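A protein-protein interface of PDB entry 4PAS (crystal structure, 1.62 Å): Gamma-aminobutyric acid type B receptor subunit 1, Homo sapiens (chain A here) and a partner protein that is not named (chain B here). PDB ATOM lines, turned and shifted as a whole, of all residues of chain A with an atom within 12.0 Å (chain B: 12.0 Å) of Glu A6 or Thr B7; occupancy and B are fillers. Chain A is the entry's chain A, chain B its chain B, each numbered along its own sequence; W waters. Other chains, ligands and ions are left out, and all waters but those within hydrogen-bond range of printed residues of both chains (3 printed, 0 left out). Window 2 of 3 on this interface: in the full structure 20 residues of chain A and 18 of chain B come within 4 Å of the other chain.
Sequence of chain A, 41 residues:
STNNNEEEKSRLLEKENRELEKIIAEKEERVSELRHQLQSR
The backbone carbonyl oxygen (O) of Leu B13 lies within hydrogen-bond range of the side-chain amide nitrogen (ND2) of Asn A17 (3.1 Å).
NH2 of Arg B9 lies within salt-bridge range of OE1 of Glu A14, 3.7 Å away.
The side-chain carboxylate (OE1) of Glu A6 lies within hydrogen-bond range of the side-chain hydroxyl (OG1) of Thr B7 (2.6 Å).
OE1 of Glu B16 lies within hydrogen-bond range of ND2 of Asn A17, at 2.9 Å.
Glu A6 touches just these residues of chain B: Thr B7 and Leu B10.
Printed residues of chain A within 4 Å of Thr B7: Glu A6.
Lys A9 touches just one residue of chain B: Leu B10.
Ser A10 touches just these residues of chain B: Arg B9, Leu B10 and Leu B13.
No residue of chain A comes within 4 Å of Gln B4.
No residue of chain A comes within 4 Å of Ala B5.
No residue of chain A comes within 4 Å of Ser B8.
No residue of chain A comes within 4 Å of Glu B11.
Printed residues of chain B within 4 Å of Leu A13: Leu B13 and Gln B14.
Of the printed residues of chain A, Gln B14 touches Leu A13 (3.6 Å).
Printed residues of chain B within 4 Å of Asn A17: Leu B13 and Glu B16.
Of the printed residues of chain A, Glu B16 touches Asn A17 (2.9 Å).
Val B2 touches none of the printed residues of chain A.
Hydrophobic or aromatic side chains of chain A within 4 Å of the printed part of chain B: Leu A13.
Printed residues of chain B that touch a printed residue of chain A: Thr B7, Arg B9, Leu B10, Leu B13, Gln B14 and Glu B16.
Hydrophobic or aromatic side chains of chain B within 4 Å of the printed part of chain A: Leu B10 and Leu B13.
Among the printed residues, 12 pairs touch across the chains.
Among the printed residues, Asp or Glu carboxylates within 4 Å of a Lys or Arg side-chain nitrogen of the other chain: Glu A14 with Arg B9 (3.7 Å).
Among the printed residues, pairs that only touch across the chains: Ser A10 with Arg B9 (3.2 Å), Glu A14 with Leu B13 (3.3 Å), Lys A9 with Leu B10 (3.4 Å), Ser A10 with Leu B10 (3.4 Å), Ser A10 with Leu B13 (3.5 Å), Leu A13 with Gln B14 (3.6 Å), Leu A13 with Leu B13 (3.7 Å) and Glu A6 with Leu B10 (3.8 Å).
Water W3 lies within hydrogen-bond range of the side-chain carboxylate of Glu A14 (2.6 Å) and the side-chain carboxylate of Glu B16 (2.7 Å).
Water W2 lies within hydrogen-bond range of O of Asn B3, OG1 of Thr B7 and OE1 of Glu A6.
Water W1 lies within hydrogen-bond range of O of Thr B7 (2.9 Å) and OE2 of Glu A6 (3.0 Å).
The side-chain hydroxyl (OG) of Ser A10 is in hydrogen-bond range of the backbone carbonyl oxygen (O) of Glu A6, at 3.2 Å.
The backbone carbonyl oxygen (O) of Leu A13 lies close to the side-chain amide oxygen (OD1) of Asn A17 (3.4 Å).
OG1 of Thr B7 lies within hydrogen-bond range of O of Asn B3.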
ATOM      1  N   GLU A   6     -10.129   6.085 -24.724  1.00  0.00           N
ATOM      2  CA  GLU A   6      -8.886   6.261 -23.919  1.00  0.00           C
ATOM      3  C   GLU A   6      -8.946   5.492 -22.597  1.00  0.00           C
ATOM      4  O   GLU A   6      -7.933   5.329 -21.916  1.00  0.00           O
ATOM      5  CB  GLU A   6      -8.616   7.749 -23.663  1.00  0.00           C
ATOM      6  CG  GLU A   6      -8.144   8.515 -24.900  1.00  0.00           C
ATOM      7  CD  GLU A   6      -7.870   9.984 -24.620  1.00  0.00           C
ATOM      8  OE1 GLU A   6      -8.619  10.584 -23.820  1.00  0.00           O
ATOM      9  OE2 GLU A   6      -6.908  10.540 -25.203  1.00  0.00           O
ATOM     10  N   GLU A   7     -10.136   5.007 -22.248  1.00  0.00           N
ATOM     11  CA  GLU A   7     -10.333   4.266 -21.002  1.00  0.00           C
ATOM     12  C   GLU A   7      -9.682   2.879 -21.058  1.00  0.00           C
ATOM     13  O   GLU A   7      -9.032   2.457 -20.095  1.00  0.00           O
ATOM     14  CB  GLU A   7     -11.828   4.171 -20.659  1.00  0.00           C
ATOM     15  CG  GLU A   7     -12.474   5.536 -20.360  1.00  0.00           C
ATOM     16  CD  GLU A   7     -13.958   5.447 -20.011  1.00  0.00           C
ATOM     17  OE1 GLU A   7     -14.297   4.909 -18.932  1.00  0.00           O
ATOM     18  OE2 GLU A   7     -14.788   5.933 -20.810  1.00  0.00           O
ATOM     19  N   GLU A   8      -9.840   2.189 -22.189  1.00  0.00           N
ATOM     20  CA  GLU A   8      -9.202   0.884 -22.402  1.00  0.00           C
ATOM     21  C   GLU A   8      -7.687   1.052 -22.408  1.00  0.00           C
ATOM     22  O   GLU A   8      -6.965   0.287 -21.766  1.00  0.00           O
ATOM     23  CB  GLU A   8      -9.640   0.259 -23.734  1.00  0.00           C
ATOM     24  CG  GLU A   8      -9.021  -1.120 -24.005  1.00  0.00           C
ATOM     25  CD  GLU A   8      -9.171  -1.580 -25.450  1.00  0.00           C
ATOM     26  OE1 GLU A   8      -8.301  -1.250 -26.286  1.00  0.00           O
ATOM     27  OE2 GLU A   8     -10.156  -2.289 -25.746  1.00  0.00           O
ATOM     28  N   LYS A   9      -7.215   2.054 -23.145  1.00  0.00           N
ATOM     29  CA  LYS A   9      -5.785   2.319 -23.247  1.00  0.00           C
ATOM     30  C   LYS A   9      -5.165   2.596 -21.882  1.00  0.00           C
ATOM     31  O   LYS A   9      -4.082   2.097 -21.580  1.00  0.00           O
ATOM     32  CB  LYS A   9      -5.506   3.491 -24.190  1.00  0.00           C
ATOM     33  CG  LYS A   9      -5.837   3.200 -25.642  1.00  0.00           C
ATOM     34  CD  LYS A   9      -4.963   4.001 -26.599  1.00  0.00           C
ATOM     35  CE  LYS A   9      -5.071   5.499 -26.360  1.00  0.00           C
ATOM     36  NZ  LYS A   9      -6.477   5.983 -26.429  1.00  0.00           N
ATOM     37  N   SER A  10      -5.851   3.387 -21.057  1.00  0.00           N
ATOM     38  CA  SER A  10      -5.340   3.699 -19.718  1.00  0.00           C
ATOM     39  C   SER A  10      -5.299   2.454 -18.844  1.00  0.00           C
ATOM     40  O   SER A  10      -4.338   2.224 -18.112  1.00  0.00           O
ATOM     41  CB  SER A  10      -6.206   4.760 -19.037  1.00  0.00           C
ATOM     42  OG  SER A  10      -5.912   6.048 -19.528  1.00  0.00           O
ATOM     43  N   ARG A  11      -6.358   1.652 -18.915  1.00  0.00           N
ATOM     44  CA  ARG A  11      -6.429   0.438 -18.126  1.00  0.00           C
ATOM     45  C   ARG A  11      -5.290  -0.505 -18.523  1.00  0.00           C
ATOM     46  O   ARG A  11      -4.627  -1.097 -17.661  1.00  0.00           O
ATOM     47  CB  ARG A  11      -7.788  -0.218 -18.344  1.00  0.00           C
ATOM     48  CG  ARG A  11      -8.010  -1.428 -17.511  1.00  0.00           C
ATOM     49  CD  ARG A  11      -9.438  -1.905 -17.676  1.00  0.00           C
ATOM     50  NE  ARG A  11      -9.616  -3.166 -16.985  1.00  0.00           N
ATOM     51  CZ  ARG A  11     -10.792  -3.732 -16.759  1.00  0.00           C
ATOM     52  NH1 ARG A  11     -11.908  -3.140 -17.168  1.00  0.00           N
ATOM     53  NH2 ARG A  11     -10.842  -4.886 -16.116  1.00  0.00           N
ATOM     54  N   LEU A  12      -5.049  -0.624 -19.826  1.00  0.00           N
ATOM     55  CA  LEU A  12      -3.978  -1.494 -20.321  1.00  0.00           C
ATOM     56  C   LEU A  12      -2.607  -0.919 -19.985  1.00  0.00           C
ATOM     57  O   LEU A  12      -1.696  -1.654 -19.598  1.00  0.00           O
ATOM     58  CB  LEU A  12      -4.089  -1.702 -21.836  1.00  0.00           C
ATOM     59  CG  LEU A  12      -5.330  -2.435 -22.356  1.00  0.00           C
ATOM     60  CD1 LEU A  12      -5.202  -2.666 -23.866  1.00  0.00           C
ATOM     61  CD2 LEU A  12      -5.526  -3.748 -21.621  1.00  0.00           C
ATOM     62  N   LEU A  13      -2.456   0.394 -20.129  1.00  0.00           N
ATOM     63  CA  LEU A  13      -1.153   1.010 -19.866  1.00  0.00           C
ATOM     64  C   LEU A  13      -0.803   0.939 -18.386  1.00  0.00           C
ATOM     65  O   LEU A  13       0.364   0.783 -18.023  1.00  0.00           O
ATOM     66  CB  LEU A  13      -1.112   2.456 -20.373  1.00  0.00           C
ATOM     67  CG  LEU A  13       0.280   3.099 -20.453  1.00  0.00           C
ATOM     68  CD1 LEU A  13       1.268   2.206 -21.204  1.00  0.00           C
ATOM     69  CD2 LEU A  13       0.172   4.447 -21.128  1.00  0.00           C
ATOM     70  N   GLU A  14      -1.811   1.060 -17.532  1.00  0.00           N
ATOM     71  CA  GLU A  14      -1.603   0.913 -16.094  1.00  0.00           C
ATOM     72  C   GLU A  14      -1.019  -0.471 -15.805  1.00  0.00           C
ATOM     73  O   GLU A  14      -0.066  -0.598 -15.033  1.00  0.00           O
ATOM     74  CB  GLU A  14      -2.930   1.098 -15.358  1.00  0.00           C
ATOM     75  CG  GLU A  14      -2.901   0.742 -13.878  1.00  0.00           C
ATOM     76  CD  GLU A  14      -2.108   1.720 -13.040  1.00  0.00           C
ATOM     77  OE1 GLU A  14      -1.914   2.875 -13.473  1.00  0.00           O
ATOM     78  OE2 GLU A  14      -1.687   1.329 -11.929  1.00  0.00           O
ATOM     79  N   LYS A  15      -1.577  -1.503 -16.437  1.00  0.00           N
ATOM     80  CA  LYS A  15      -1.065  -2.864 -16.243  1.00  0.00           C
ATOM     81  C   LYS A  15       0.349  -3.031 -16.808  1.00  0.00           C
ATOM     82  O   LYS A  15       1.174  -3.734 -16.220  1.00  0.00           O
ATOM     83  CB  LYS A  15      -2.015  -3.902 -16.863  1.00  0.00           C
ATOM     84  CG  LYS A  15      -3.372  -4.022 -16.143  1.00  0.00           C
ATOM     85  CD  LYS A  15      -3.190  -4.389 -14.663  1.00  0.00           C
ATOM     86  CE  LYS A  15      -4.511  -4.661 -13.960  1.00  0.00           C
ATOM     87  NZ  LYS A  15      -5.430  -3.489 -13.983  1.00  0.00           N
ATOM     88  N   ASN A  17       2.626  -0.641 -17.044  1.00  0.00           N
ATOM     89  CA  ASN A  17       3.533   0.046 -16.133  1.00  0.00           C
ATOM     90  C   ASN A  17       3.808  -0.789 -14.888  1.00  0.00           C
ATOM     91  O   ASN A  17       4.938  -0.848 -14.403  1.00  0.00           O
ATOM     92  CB  ASN A  17       2.956   1.413 -15.750  1.00  0.00           C
ATOM     93  CG  ASN A  17       2.982   2.397 -16.901  1.00  0.00           C
ATOM     94  OD1 ASN A  17       3.508   2.094 -17.980  1.00  0.00           O
ATOM     95  ND2 ASN A  17       2.441   3.584 -16.681  1.00  0.00           N
ATOM     96  N   SER B   1     -16.450  16.732 -17.406  1.00  0.00           N
ATOM     97  CA  SER B   1     -15.022  16.996 -17.084  1.00  0.00           C
ATOM     98  C   SER B   1     -14.302  15.691 -16.752  1.00  0.00           C
ATOM     99  O   SER B   1     -13.076  15.650 -16.679  1.00  0.00           O
ATOM    100  CB  SER B   1     -14.905  18.000 -15.947  1.00  0.00           C
ATOM    101  OG  SER B   1     -13.626  18.588 -15.931  1.00  0.00           O
ATOM    102  N   VAL B   2     -15.072  14.618 -16.578  1.00  0.00           N
ATOM    103  CA  VAL B   2     -14.483  13.289 -16.397  1.00  0.00           C
ATOM    104  C   VAL B   2     -13.793  12.834 -17.687  1.00  0.00           C
ATOM    105  O   VAL B   2     -12.893  11.994 -17.650  1.00  0.00           O
ATOM    106  CB  VAL B   2     -15.525  12.218 -15.977  1.00  0.00           C
ATOM    107  CG1 VAL B   2     -15.964  12.426 -14.520  1.00  0.00           C
ATOM    108  CG2 VAL B   2     -16.722  12.218 -16.924  1.00  0.00           C
ATOM    109  N   ASN B   3     -14.211  13.392 -18.825  1.00  0.00           N
ATOM    110  CA  ASN B   3     -13.592  13.053 -20.109  1.00  0.00           C
ATOM    111  C   ASN B   3     -12.193  13.641 -20.189  1.00  0.00           C
ATOM    112  O   ASN B   3     -11.254  12.983 -20.655  1.00  0.00           O
ATOM    113  CB  ASN B   3     -14.440  13.565 -21.277  1.00  0.00           C
ATOM    114  CG  ASN B   3     -15.829  12.960 -21.296  1.00  0.00           C
ATOM    115  OD1 ASN B   3     -16.816  13.655 -21.547  1.00  0.00           O
ATOM    116  ND2 ASN B   3     -15.915  11.666 -21.028  1.00  0.00           N
ATOM    117  N   GLN B   4     -12.058  14.886 -19.741  1.00  0.00           N
ATOM    118  CA  GLN B   4     -10.755  15.541 -19.698  1.00  0.00           C
ATOM    119  C   GLN B   4      -9.864  14.844 -18.673  1.00  0.00           C
ATOM    120  O   GLN B   4      -8.655  14.694 -18.889  1.00  0.00           O
ATOM    121  CB  GLN B   4     -10.898  17.033 -19.380  1.00  0.00           C
ATOM    122  CG  GLN B   4     -11.462  17.866 -20.542  1.00  0.00           C
ATOM    123  CD  GLN B   4     -10.507  17.982 -21.731  1.00  0.00           C
ATOM    124  OE1 GLN B   4      -9.519  17.262 -21.811  1.00  0.00           O
ATOM    125  NE2 GLN B   4     -10.802  18.879 -22.659  1.00  0.00           N
ATOM    126  N   ALA B   5     -10.466  14.392 -17.573  1.00  0.00           N
ATOM    127  CA  ALA B   5      -9.723  13.670 -16.543  1.00  0.00           C
ATOM    128  C   ALA B   5      -9.128  12.396 -17.123  1.00  0.00           C
ATOM    129  O   ALA B   5      -7.973  12.059 -16.854  1.00  0.00           O
ATOM    130  CB  ALA B   5     -10.629  13.343 -15.370  1.00  0.00           C
ATOM    131  N   SER B   6      -9.916  11.689 -17.929  1.00  0.00           N
ATOM    132  CA  SER B   6      -9.446  10.446 -18.545  1.00  0.00           C
ATOM    133  C   SER B   6      -8.284  10.702 -19.500  1.00  0.00           C
ATOM    134  O   SER B   6      -7.340   9.918 -19.574  1.00  0.00           O
ATOM    135  CB  SER B   6     -10.587   9.750 -19.286  1.00  0.00           C
ATOM    136  OG  SER B   6     -11.456   9.111 -18.365  1.00  0.00           O
ATOM    137  N   THR B   7      -8.354  11.814 -20.225  1.00  0.00           N
ATOM    138  CA  THR B   7      -7.295  12.169 -21.156  1.00  0.00           C
ATOM    139  C   THR B   7      -6.004  12.472 -20.409  1.00  0.00           C
ATOM    140  O   THR B   7      -4.925  12.036 -20.817  1.00  0.00           O
ATOM    141  CB  THR B   7      -7.730  13.359 -22.016  1.00  0.00           C
ATOM    142  OG1 THR B   7      -8.832  12.945 -22.826  1.00  0.00           O
ATOM    143  CG2 THR B   7      -6.591  13.836 -22.920  1.00  0.00           C
ATOM    144  N   SER B   8      -6.121  13.204 -19.305  1.00  0.00           N
ATOM    145  CA  SER B   8      -4.962  13.523 -18.475  1.00  0.00           C
ATOM    146  C   SER B   8      -4.375  12.253 -17.894  1.00  0.00           C
ATOM    147  O   SER B   8      -3.157  12.103 -17.834  1.00  0.00           O
ATOM    148  CB  SER B   8      -5.352  14.471 -17.340  1.00  0.00           C
ATOM    149  OG  SER B   8      -5.675  15.755 -17.839  1.00  0.00           O
ATOM    150  N   ARG B   9      -5.242  11.345 -17.446  1.00  0.00           N
ATOM    151  CA  ARG B   9      -4.769  10.082 -16.878  1.00  0.00           C
ATOM    152  C   ARG B   9      -3.893   9.334 -17.884  1.00  0.00           C
ATOM    153  O   ARG B   9      -2.794   8.875 -17.549  1.00  0.00           O
ATOM    154  CB  ARG B   9      -5.950   9.197 -16.443  1.00  0.00           C
ATOM    155  CG  ARG B   9      -5.496   7.902 -15.758  1.00  0.00           C
ATOM    156  CD  ARG B   9      -6.654   7.039 -15.271  1.00  0.00           C
ATOM    157  NE  ARG B   9      -6.180   6.021 -14.332  1.00  0.00           N
ATOM    158  CZ  ARG B   9      -5.957   4.742 -14.632  1.00  0.00           C
ATOM    159  NH1 ARG B   9      -6.176   4.282 -15.858  1.00  0.00           N
ATOM    160  NH2 ARG B   9      -5.507   3.916 -13.696  1.00  0.00           N
ATOM    161  N   LEU B  10      -4.369   9.222 -19.120  1.00  0.00           N
ATOM    162  CA  LEU B  10      -3.605   8.526 -20.156  1.00  0.00           C
ATOM    163  C   LEU B  10      -2.260   9.198 -20.415  1.00  0.00           C
ATOM    164  O   LEU B  10      -1.235   8.519 -20.522  1.00  0.00           O
ATOM    165  CB  LEU B  10      -4.401   8.434 -21.461  1.00  0.00           C
ATOM    166  CG  LEU B  10      -3.697   7.666 -22.586  1.00  0.00           C
ATOM    167  CD1 LEU B  10      -3.381   6.237 -22.151  1.00  0.00           C
ATOM    168  CD2 LEU B  10      -4.589   7.665 -23.830  1.00  0.00           C
ATOM    169  N   GLU B  11      -2.257  10.523 -20.521  1.00  0.00           N
ATOM    170  CA  GLU B  11      -0.999  11.241 -20.758  1.00  0.00           C
ATOM    171  C   GLU B  11      -0.019  11.001 -19.622  1.00  0.00           C
ATOM    172  O   GLU B  11       1.180  10.811 -19.854  1.00  0.00           O
ATOM    173  CB  GLU B  11      -1.243  12.742 -20.939  1.00  0.00           C
ATOM    174  CG  GLU B  11      -2.055  13.076 -22.174  1.00  0.00           C
ATOM    175  CD  GLU B  11      -2.164  14.566 -22.435  1.00  0.00           C
ATOM    176  OE1 GLU B  11      -2.248  15.339 -21.461  1.00  0.00           O
ATOM    177  OE2 GLU B  11      -2.181  14.963 -23.620  1.00  0.00           O
ATOM    178  N   GLY B  12      -0.529  11.015 -18.392  1.00  0.00           N
ATOM    179  CA  GLY B  12       0.312  10.768 -17.224  1.00  0.00           C
ATOM    180  C   GLY B  12       0.891   9.366 -17.237  1.00  0.00           C
ATOM    181  O   GLY B  12       2.061   9.168 -16.910  1.00  0.00           O
ATOM    182  N   LEU B  13       0.075   8.386 -17.622  1.00  0.00           N
ATOM    183  CA  LEU B  13       0.565   7.008 -17.668  1.00  0.00           C
ATOM    184  C   LEU B  13       1.609   6.846 -18.763  1.00  0.00           C
ATOM    185  O   LEU B  13       2.519   6.019 -18.640  1.00  0.00           O
ATOM    186  CB  LEU B  13      -0.597   6.030 -17.865  1.00  0.00           C
ATOM    187  CG  LEU B  13      -1.555   5.927 -16.679  1.00  0.00           C
ATOM    188  CD1 LEU B  13      -2.831   5.198 -17.099  1.00  0.00           C
ATOM    189  CD2 LEU B  13      -0.872   5.217 -15.515  1.00  0.00           C
ATOM    190  N   GLN B  14       1.487   7.630 -19.834  1.00  0.00           N
ATOM    191  CA  GLN B  14       2.477   7.581 -20.916  1.00  0.00           C
ATOM    192  C   GLN B  14       3.809   8.157 -20.436  1.00  0.00           C
ATOM    193  O   GLN B  14       4.888   7.643 -20.771  1.00  0.00           O
ATOM    194  CB  GLN B  14       1.963   8.331 -22.153  1.00  0.00           C
ATOM    195  CG  GLN B  14       0.794   7.612 -22.821  1.00  0.00           C
ATOM    196  CD  GLN B  14       0.189   8.371 -23.993  1.00  0.00           C
ATOM    197  OE1 GLN B  14       0.151   9.602 -24.007  1.00  0.00           O
ATOM    198  NE2 GLN B  14      -0.308   7.628 -24.978  1.00  0.00           N
ATOM    199  N   SER B  15       3.735   9.213 -19.632  1.00  0.00           N
ATOM    200  CA  SER B  15       4.939   9.814 -19.055  1.00  0.00           C
ATOM    201  C   SER B  15       5.595   8.804 -18.126  1.00  0.00           C
ATOM    202  O   SER B  15       6.818   8.617 -18.156  1.00  0.00           O
ATOM    203  CB  SER B  15       4.600  11.081 -18.268  1.00  0.00           C
ATOM    204  OG  SER B  15       4.164  12.119 -19.133  1.00  0.00           O
ATOM    205  N   GLU B  16       4.784   8.153 -17.300  1.00  0.00           N
ATOM    206  CA  GLU B  16       5.293   7.154 -16.370  1.00  0.00           C
ATOM    207  C   GLU B  16       5.945   5.997 -17.127  1.00  0.00           C
ATOM    208  O   GLU B  16       7.008   5.512 -16.746  1.00  0.00           O
ATOM    209  CB  GLU B  16       4.159   6.632 -15.482  1.00  0.00           C
ATOM    210  CG  GLU B  16       4.624   5.602 -14.453  1.00  0.00           C
ATOM    211  CD  GLU B  16       3.505   5.077 -13.587  1.00  0.00           C
ATOM    212  OE1 GLU B  16       2.386   4.853 -14.105  1.00  0.00           O
ATOM    213  OE2 GLU B  16       3.744   4.863 -12.375  1.00  0.00           O
HETATM  214  O   HOH W   1      -4.526  11.204 -23.586  1.00  0.00           O
HETATM  215  O   HOH W   2     -11.502  11.299 -22.753  1.00  0.00           O
HETATM  216  O   HOH W   3       0.413   3.752 -12.625  1.00  0.00           O
